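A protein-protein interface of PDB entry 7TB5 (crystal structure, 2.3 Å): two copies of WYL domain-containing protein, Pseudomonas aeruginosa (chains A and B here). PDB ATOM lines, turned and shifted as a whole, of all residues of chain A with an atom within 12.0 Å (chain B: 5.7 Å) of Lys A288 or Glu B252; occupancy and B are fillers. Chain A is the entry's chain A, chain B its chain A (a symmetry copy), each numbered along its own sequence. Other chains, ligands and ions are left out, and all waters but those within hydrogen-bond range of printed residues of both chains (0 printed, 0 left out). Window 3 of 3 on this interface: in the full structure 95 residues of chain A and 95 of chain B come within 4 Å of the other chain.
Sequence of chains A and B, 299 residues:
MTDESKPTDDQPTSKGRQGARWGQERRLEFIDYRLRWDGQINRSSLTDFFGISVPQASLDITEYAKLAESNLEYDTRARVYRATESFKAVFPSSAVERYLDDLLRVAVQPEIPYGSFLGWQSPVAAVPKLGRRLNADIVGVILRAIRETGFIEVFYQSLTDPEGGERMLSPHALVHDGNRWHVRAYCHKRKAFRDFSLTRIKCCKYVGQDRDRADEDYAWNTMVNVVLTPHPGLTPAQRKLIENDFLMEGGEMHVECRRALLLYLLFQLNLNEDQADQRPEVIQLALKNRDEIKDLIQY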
ATOM      1  N   LEU A 130     -11.495  14.128  -2.553  1.00  0.00           N
ATOM      2  CA  LEU A 130     -11.030  12.802  -2.162  1.00  0.00           C
ATOM      3  C   LEU A 130     -11.730  11.690  -2.945  1.00  0.00           C
ATOM      4  O   LEU A 130     -11.186  10.588  -3.088  1.00  0.00           O
ATOM      5  CB  LEU A 130     -11.260  12.605  -0.663  1.00  0.00           C
ATOM      6  CG  LEU A 130     -10.397  13.396   0.306  1.00  0.00           C
ATOM      7  CD1 LEU A 130     -10.793  13.075   1.738  1.00  0.00           C
ATOM      8  CD2 LEU A 130      -8.929  13.078   0.056  1.00  0.00           C
ATOM      9  N   VAL A 282     -15.823   7.992   0.930  1.00  0.00           N
ATOM     10  CA  VAL A 282     -14.840   8.879   1.541  1.00  0.00           C
ATOM     11  C   VAL A 282     -15.083   9.027   3.030  1.00  0.00           C
ATOM     12  O   VAL A 282     -14.133   9.141   3.803  1.00  0.00           O
ATOM     13  CB  VAL A 282     -14.858  10.244   0.828  1.00  0.00           C
ATOM     14  CG1 VAL A 282     -14.196  11.305   1.678  1.00  0.00           C
ATOM     15  CG2 VAL A 282     -14.176  10.136  -0.553  1.00  0.00           C
ATOM     16  N   ILE A 283     -16.348   9.020   3.461  1.00  0.00           N
ATOM     17  CA  ILE A 283     -16.664   9.122   4.883  1.00  0.00           C
ATOM     18  C   ILE A 283     -16.012   8.014   5.697  1.00  0.00           C
ATOM     19  O   ILE A 283     -15.852   8.151   6.917  1.00  0.00           O
ATOM     20  CB  ILE A 283     -18.198   9.098   5.073  1.00  0.00           C
ATOM     21  CG1 ILE A 283     -18.824  10.315   4.389  1.00  0.00           C
ATOM     22  CG2 ILE A 283     -18.551   9.040   6.537  1.00  0.00           C
ATOM     23  CD1 ILE A 283     -20.335  10.381   4.495  1.00  0.00           C
ATOM     24  N   GLN A 284     -15.635   6.915   5.049  1.00  0.00           N
ATOM     25  CA  GLN A 284     -15.107   5.743   5.729  1.00  0.00           C
ATOM     26  C   GLN A 284     -13.584   5.738   5.783  1.00  0.00           C
ATOM     27  O   GLN A 284     -12.974   4.707   6.102  1.00  0.00           O
ATOM     28  CB  GLN A 284     -15.642   4.489   5.045  1.00  0.00           C
ATOM     29  CG  GLN A 284     -17.159   4.479   4.924  1.00  0.00           C
ATOM     30  CD  GLN A 284     -17.834   4.187   6.254  1.00  0.00           C
ATOM     31  OE1 GLN A 284     -17.499   3.204   6.922  1.00  0.00           O
ATOM     32  NE2 GLN A 284     -18.795   5.030   6.643  1.00  0.00           N
ATOM     33  N   LEU A 285     -12.964   6.883   5.525  1.00  0.00           N
ATOM     34  CA  LEU A 285     -11.547   7.071   5.771  1.00  0.00           C
ATOM     35  C   LEU A 285     -11.337   7.644   7.163  1.00  0.00           C
ATOM     36  O   LEU A 285     -12.285   7.983   7.874  1.00  0.00           O
ATOM     37  CB  LEU A 285     -10.940   8.006   4.728  1.00  0.00           C
ATOM     38  CG  LEU A 285     -11.073   7.581   3.262  1.00  0.00           C
ATOM     39  CD1 LEU A 285     -10.674   8.709   2.320  1.00  0.00           C
ATOM     40  CD2 LEU A 285     -10.225   6.344   3.012  1.00  0.00           C
ATOM     41  N   ALA A 286     -10.070   7.764   7.547  1.00  0.00           N
ATOM     42  CA  ALA A 286      -9.725   8.391   8.810  1.00  0.00           C
ATOM     43  C   ALA A 286      -8.347   9.026   8.699  1.00  0.00           C
ATOM     44  O   ALA A 286      -7.484   8.556   7.955  1.00  0.00           O
ATOM     45  CB  ALA A 286      -9.746   7.395   9.980  1.00  0.00           C
ATOM     46  N   LEU A 287      -8.146  10.086   9.473  1.00  0.00           N
ATOM     47  CA  LEU A 287      -6.858  10.763   9.493  1.00  0.00           C
ATOM     48  C   LEU A 287      -5.853   9.964  10.300  1.00  0.00           C
ATOM     49  O   LEU A 287      -6.106   9.623  11.459  1.00  0.00           O
ATOM     50  CB  LEU A 287      -6.994  12.153  10.107  1.00  0.00           C
ATOM     51  CG  LEU A 287      -7.565  13.267   9.245  1.00  0.00           C
ATOM     52  CD1 LEU A 287      -7.940  14.431  10.142  1.00  0.00           C
ATOM     53  CD2 LEU A 287      -6.564  13.677   8.192  1.00  0.00           C
ATOM     54  N   LYS A 288      -4.693   9.697   9.700  1.00  0.00           N
ATOM     55  CA  LYS A 288      -3.617   9.066  10.454  1.00  0.00           C
ATOM     56  C   LYS A 288      -3.280   9.898  11.685  1.00  0.00           C
ATOM     57  O   LYS A 288      -3.155   9.370  12.801  1.00  0.00           O
ATOM     58  CB  LYS A 288      -2.392   8.891   9.553  1.00  0.00           C
ATOM     59  CG  LYS A 288      -1.178   8.237  10.216  1.00  0.00           C
ATOM     60  CD  LYS A 288       0.031   8.201   9.264  1.00  0.00           C
ATOM     61  CE  LYS A 288       1.273   7.631   9.949  1.00  0.00           C
ATOM     62  NZ  LYS A 288       2.439   7.534   9.019  1.00  0.00           N
ATOM     63  N   ASN A 289      -3.136  11.210  11.499  1.00  0.00           N
ATOM     64  CA  ASN A 289      -2.738  12.125  12.569  1.00  0.00           C
ATOM     65  C   ASN A 289      -3.853  13.140  12.786  1.00  0.00           C
ATOM     66  O   ASN A 289      -3.789  14.263  12.284  1.00  0.00           O
ATOM     67  CB  ASN A 289      -1.402  12.832  12.237  1.00  0.00           C
ATOM     68  CG  ASN A 289      -0.311  11.862  11.847  1.00  0.00           C
ATOM     69  OD1 ASN A 289       0.356  11.261  12.711  1.00  0.00           O
ATOM     70  ND2 ASN A 289      -0.108  11.706  10.535  1.00  0.00           N
ATOM     71  N   ARG A 290      -4.875  12.744  13.549  1.00  0.00           N
ATOM     72  CA  ARG A 290      -5.979  13.660  13.821  1.00  0.00           C
ATOM     73  C   ARG A 290      -5.555  14.775  14.775  1.00  0.00           C
ATOM     74  O   ARG A 290      -6.100  15.886  14.715  1.00  0.00           O
ATOM     75  CB  ARG A 290      -7.174  12.890  14.386  1.00  0.00           C
ATOM     76  N   ASP A 291      -4.582  14.509  15.651  1.00  0.00           N
ATOM     77  CA  ASP A 291      -4.120  15.545  16.570  1.00  0.00           C
ATOM     78  C   ASP A 291      -3.339  16.633  15.829  1.00  0.00           C
ATOM     79  O   ASP A 291      -3.566  17.833  16.045  1.00  0.00           O
ATOM     80  CB  ASP A 291      -3.266  14.917  17.673  1.00  0.00           C
ATOM     81  N   GLU A 292      -2.429  16.232  14.939  1.00  0.00           N
ATOM     82  CA  GLU A 292      -1.557  17.198  14.276  1.00  0.00           C
ATOM     83  C   GLU A 292      -2.317  18.024  13.240  1.00  0.00           C
ATOM     84  O   GLU A 292      -2.032  19.209  13.057  1.00  0.00           O
ATOM     85  CB  GLU A 292      -0.374  16.452  13.653  1.00  0.00           C
ATOM     86  CG  GLU A 292       0.318  17.154  12.517  1.00  0.00           C
ATOM     87  CD  GLU A 292       1.101  16.166  11.625  1.00  0.00           C
ATOM     88  OE1 GLU A 292       1.738  15.229  12.186  1.00  0.00           O
ATOM     89  OE2 GLU A 292       1.054  16.317  10.372  1.00  0.00           O
ATOM     90  N   ILE A 293      -3.263  17.422  12.529  1.00  0.00           N
ATOM     91  CA  ILE A 293      -3.997  18.183  11.525  1.00  0.00           C
ATOM     92  C   ILE A 293      -5.023  19.106  12.181  1.00  0.00           C
ATOM     93  O   ILE A 293      -5.398  20.132  11.604  1.00  0.00           O
ATOM     94  CB  ILE A 293      -4.643  17.208  10.525  1.00  0.00           C
ATOM     95  CG1 ILE A 293      -3.800  17.086   9.245  1.00  0.00           C
ATOM     96  CG2 ILE A 293      -6.045  17.665  10.135  1.00  0.00           C
ATOM     97  CD1 ILE A 293      -2.329  16.796   9.471  1.00  0.00           C
ATOM     98  N   LYS A 294      -5.488  18.771  13.385  1.00  0.00           N
ATOM     99  CA  LYS A 294      -6.428  19.648  14.072  1.00  0.00           C
ATOM    100  C   LYS A 294      -5.738  20.927  14.517  1.00  0.00           C
ATOM    101  O   LYS A 294      -6.318  22.017  14.432  1.00  0.00           O
ATOM    102  CB  LYS A 294      -7.039  18.936  15.276  1.00  0.00           C
ATOM    103  N   ASP A 295      -4.492  20.811  14.992  1.00  0.00           N
ATOM    104  CA  ASP A 295      -3.734  21.996  15.385  1.00  0.00           C
ATOM    105  C   ASP A 295      -3.634  22.995  14.239  1.00  0.00           C
ATOM    106  O   ASP A 295      -3.693  24.214  14.453  1.00  0.00           O
ATOM    107  CB  ASP A 295      -2.331  21.598  15.849  1.00  0.00           C
ATOM    108  CG  ASP A 295      -2.345  20.802  17.142  1.00  0.00           C
ATOM    109  OD1 ASP A 295      -3.431  20.712  17.762  1.00  0.00           O
ATOM    110  OD2 ASP A 295      -1.279  20.265  17.541  1.00  0.00           O
ATOM    111  N   LEU A 296      -3.479  22.496  13.016  1.00  0.00           N
ATOM    112  CA  LEU A 296      -3.243  23.360  11.872  1.00  0.00           C
ATOM    113  C   LEU A 296      -4.485  24.102  11.402  1.00  0.00           C
ATOM    114  O   LEU A 296      -4.358  25.003  10.563  1.00  0.00           O
ATOM    115  CB  LEU A 296      -2.676  22.540  10.720  1.00  0.00           C
ATOM    116  CG  LEU A 296      -1.345  21.858  11.029  1.00  0.00           C
ATOM    117  CD1 LEU A 296      -0.949  20.944   9.859  1.00  0.00           C
ATOM    118  CD2 LEU A 296      -0.277  22.869  11.318  1.00  0.00           C
ATOM    119  N   VAL B 227      -2.274  12.617   5.518  1.00  0.00           N
ATOM    120  CA  VAL B 227      -2.214  11.169   5.381  1.00  0.00           C
ATOM    121  C   VAL B 227      -3.541  10.591   5.839  1.00  0.00           C
ATOM    122  O   VAL B 227      -3.947  10.802   6.989  1.00  0.00           O
ATOM    123  CB  VAL B 227      -1.059  10.578   6.201  1.00  0.00           C
ATOM    124  CG1 VAL B 227      -0.961   9.085   5.970  1.00  0.00           C
ATOM    125  CG2 VAL B 227       0.246  11.264   5.843  1.00  0.00           C
ATOM    126  N   LEU B 228      -4.189   9.826   4.958  1.00  0.00           N
ATOM    127  CA  LEU B 228      -5.438   9.138   5.262  1.00  0.00           C
ATOM    128  C   LEU B 228      -5.215   7.631   5.261  1.00  0.00           C
ATOM    129  O   LEU B 228      -4.436   7.112   4.455  1.00  0.00           O
ATOM    130  CB  LEU B 228      -6.529   9.492   4.246  1.00  0.00           C
ATOM    131  CG  LEU B 228      -6.818  10.979   4.024  1.00  0.00           C
ATOM    132  CD1 LEU B 228      -7.764  11.176   2.863  1.00  0.00           C
ATOM    133  CD2 LEU B 228      -7.380  11.630   5.258  1.00  0.00           C
ATOM    134  N   THR B 229      -5.890   6.936   6.170  1.00  0.00           N
ATOM    135  CA  THR B 229      -5.902   5.481   6.237  1.00  0.00           C
ATOM    136  C   THR B 229      -7.343   5.001   6.238  1.00  0.00           C
ATOM    137  O   THR B 229      -8.274   5.796   6.380  1.00  0.00           O
ATOM    138  CB  THR B 229      -5.195   4.966   7.500  1.00  0.00           C
ATOM    139  OG1 THR B 229      -6.054   5.162   8.632  1.00  0.00           O
ATOM    140  CG2 THR B 229      -3.873   5.697   7.697  1.00  0.00           C
ATOM    141  N   PRO B 230      -7.567   3.695   6.085  1.00  0.00           N
ATOM    142  CA  PRO B 230      -8.932   3.176   6.253  1.00  0.00           C
ATOM    143  C   PRO B 230      -9.391   3.330   7.696  1.00  0.00           C
ATOM    144  O   PRO B 230      -8.624   3.099   8.633  1.00  0.00           O
ATOM    145  CB  PRO B 230      -8.808   1.699   5.859  1.00  0.00           C
ATOM    146  CG  PRO B 230      -7.525   1.603   5.084  1.00  0.00           C
ATOM    147  CD  PRO B 230      -6.622   2.636   5.692  1.00  0.00           C
ATOM    148  N   LEU B 247      -6.560   3.397  -4.129  1.00  0.00           N
ATOM    149  CA  LEU B 247      -5.211   3.187  -4.651  1.00  0.00           C
ATOM    150  C   LEU B 247      -4.154   3.477  -3.592  1.00  0.00           C
ATOM    151  O   LEU B 247      -3.167   4.176  -3.832  1.00  0.00           O
ATOM    152  CB  LEU B 247      -4.980   4.041  -5.902  1.00  0.00           C
ATOM    153  CG  LEU B 247      -5.982   3.788  -7.038  1.00  0.00           C
ATOM    154  CD1 LEU B 247      -5.603   4.581  -8.273  1.00  0.00           C
ATOM    155  CD2 LEU B 247      -6.071   2.316  -7.345  1.00  0.00           C
ATOM    156  N   MET B 248      -4.352   2.900  -2.417  1.00  0.00           N
ATOM    157  CA  MET B 248      -3.427   3.115  -1.327  1.00  0.00           C
ATOM    158  C   MET B 248      -2.237   2.190  -1.423  1.00  0.00           C
ATOM    159  O   MET B 248      -2.355   1.062  -1.891  1.00  0.00           O
ATOM    160  CB  MET B 248      -4.124   2.911   0.013  1.00  0.00           C
ATOM    161  CG  MET B 248      -5.435   3.663   0.142  1.00  0.00           C
ATOM    162  SD  MET B 248      -6.143   3.569   1.969  1.00  0.00           S
ATOM    163  CE  MET B 248      -7.574   4.899   1.691  1.00  0.00           C
ATOM    164  N   GLU B 249      -1.086   2.682  -0.978  1.00  0.00           N
ATOM    165  CA  GLU B 249       0.127   1.890  -0.844  1.00  0.00           C
ATOM    166  C   GLU B 249       0.384   1.684   0.645  1.00  0.00           C
ATOM    167  O   GLU B 249       0.535   2.659   1.391  1.00  0.00           O
ATOM    168  CB  GLU B 249       1.303   2.598  -1.515  1.00  0.00           C
ATOM    169  N   GLY B 250       0.430   0.426   1.073  1.00  0.00           N
ATOM    170  CA  GLY B 250       0.680   0.148   2.476  1.00  0.00           C
ATOM    171  C   GLY B 250      -0.389   0.676   3.407  1.00  0.00           C
ATOM    172  O   GLY B 250      -0.077   1.086   4.531  1.00  0.00           O
ATOM    173  N   GLY B 251      -1.645   0.679   2.965  1.00  0.00           N
ATOM    174  CA  GLY B 251      -2.730   1.146   3.803  1.00  0.00           C
ATOM    175  C   GLY B 251      -2.715   2.630   4.064  1.00  0.00           C
ATOM    176  O   GLY B 251      -3.178   3.071   5.121  1.00  0.00           O
ATOM    177  N   GLU B 252      -2.205   3.419   3.123  1.00  0.00           N
ATOM    178  CA  GLU B 252      -2.084   4.854   3.314  1.00  0.00           C
ATOM    179  C   GLU B 252      -2.340   5.578   1.999  1.00  0.00           C
ATOM    180  O   GLU B 252      -2.146   5.037   0.914  1.00  0.00           O
ATOM    181  CB  GLU B 252      -0.698   5.250   3.845  1.00  0.00           C
ATOM    182  CG  GLU B 252      -0.514   5.105   5.356  1.00  0.00           C
ATOM    183  CD  GLU B 252       0.850   5.600   5.819  1.00  0.00           C
ATOM    184  OE1 GLU B 252       1.591   6.173   4.980  1.00  0.00           O
ATOM    185  OE2 GLU B 252       1.179   5.416   7.017  1.00  0.00           O
ATOM    186  N   MET B 253      -2.712   6.839   2.118  1.00  0.00           N
ATOM    187  CA  MET B 253      -3.064   7.688   0.985  1.00  0.00           C
ATOM    188  C   MET B 253      -2.570   9.083   1.341  1.00  0.00           C
ATOM    189  O   MET B 253      -2.634   9.475   2.509  1.00  0.00           O
ATOM    190  CB  MET B 253      -4.553   7.658   0.767  1.00  0.00           C
ATOM    191  CG  MET B 253      -5.063   8.546  -0.308  1.00  0.00           C
ATOM    192  SD  MET B 253      -6.996   8.542  -0.050  1.00  0.00           S
ATOM    193  CE  MET B 253      -7.530   9.634  -1.603  1.00  0.00           C
ATOM    194  N   HIS B 254      -2.056   9.819   0.356  1.00  0.00           N
ATOM    195  CA  HIS B 254      -1.460  11.133   0.577  1.00  0.00           C
ATOM    196  C   HIS B 254      -2.157  12.173  -0.284  1.00  0.00           C
ATOM    197  O   HIS B 254      -2.343  11.971  -1.490  1.00  0.00           O
ATOM    198  CB  HIS B 254       0.038  11.128   0.260  1.00  0.00           C
ATOM    199  CG  HIS B 254       0.870  10.436   1.293  1.00  0.00           C
ATOM    200  ND1 HIS B 254       1.545  11.116   2.283  1.00  0.00           N
ATOM    201  CD2 HIS B 254       1.145   9.125   1.485  1.00  0.00           C
ATOM    202  CE1 HIS B 254       2.197  10.254   3.044  1.00  0.00           C
ATOM    203  NE2 HIS B 254       1.966   9.037   2.585  1.00  0.00           N
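N of Thr B229 is in hydrogen-bond range of O of Ala A286 (2.9 Å). N of Lys A288 is in hydrogen-bond range of O of Val B227, 3.0 Å away. The side-chain carboxylate (OE2) of Glu B252 lies within salt-bridge range of the side-chain amino group (NZ) of Lys A288 (3.2 Å).
The backbone NH (N) of Met B253 sits at hydrogen-bond distance from the backbone carbonyl oxygen (O) of Leu B228, 2.9 Å away.
Leu B228 touches Leu A130 (CD1 to CD2, 3.6 Å). Leu B228 touches Leu A285. Leu A285 touches Thr B229 (CA to O, 3.6 Å). Leu A285 touches Met B248. O of Ala A286 touches CA of Leu B228, 3.4 Å away. Leu A287 touches Val B227 (CA to O, 3.8 Å). Leu A287 touches Leu B228 (CD2 to CD2, 3.7 Å). CG2 of Thr B229 touches CB of Lys A288, at 3.98 Å.
Of the printed residues of chain B, Leu A130 touches Leu B228 (3.6 Å). Val A282 touches none of the printed residues of chain B. Gln A284 touches none of the printed residues of chain B. Printed residues of chain B within 4 Å of Leu A285: Leu B228 (3.9 Å), Thr B229 (3.6 Å) and Met B248 (3.3 Å). Of the printed residues of chain B, Ala A286 touches Leu B228 (3.4 Å) and Thr B229 (2.9 Å). Printed residues of chain B within 4 Å of Leu A287: Val B227 and Leu B228. Printed residues of chain B within 4 Å of Lys A288: Val B227 (3.0 Å), Thr B229 (3.98 Å) and Glu B252 (3.2 Å). Of the printed residues of chain A, Val B227 touches Leu A287 and Lys A288. Of the printed residues of chain A, Thr B229 touches Leu A285 (3.6 Å), Ala A286 (2.9 Å) and Lys A288 (3.98 Å). Met B248 touches just one residue of chain A: Leu A285 (3.3 Å). Glu B249 touches none of the printed residues of chain A. Gly B251 touches none of the printed residues of chain A. Glu B252 touches just one residue of chain A: Lys A288 (3.2 Å). No residue of chain A comes within 4 Å of Met B253. No residue of chain A comes within 4 Å of His B254. The nearest residue of chain B that does not touch Lys A288 is Leu B228 (4.5 Å). The nearest residue of chain A that does not touch Glu B252 is Asn A289 (7.3 Å). The nearest printed residue of chain B that does not touch Leu A287 is Thr B229 (5.1 Å).
Printed residues of chain B that touch a printed residue of chain A: Val B227, Leu B228, Thr B229, Met B248 and Glu B252. Of the 16 printed residues of chain A, 5 touch a printed residue of chain B. Hydrophobic or aromatic side chains of chain A within 4 Å of the printed part of chain B: Leu A130, Leu A285 and Leu A287. Among the printed residues, 11 pairs touch across the chains. Among the printed residues, Asp or Glu carboxylates within 4 Å of a Lys or Arg side-chain nitrogen of the other chain: Lys A288 with Glu B252 (3.2 Å).
No position is printed for both chains. Of the 11 pairs that touch across the chains among the printed residues, none has its exchanged pair printed and touching as well.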
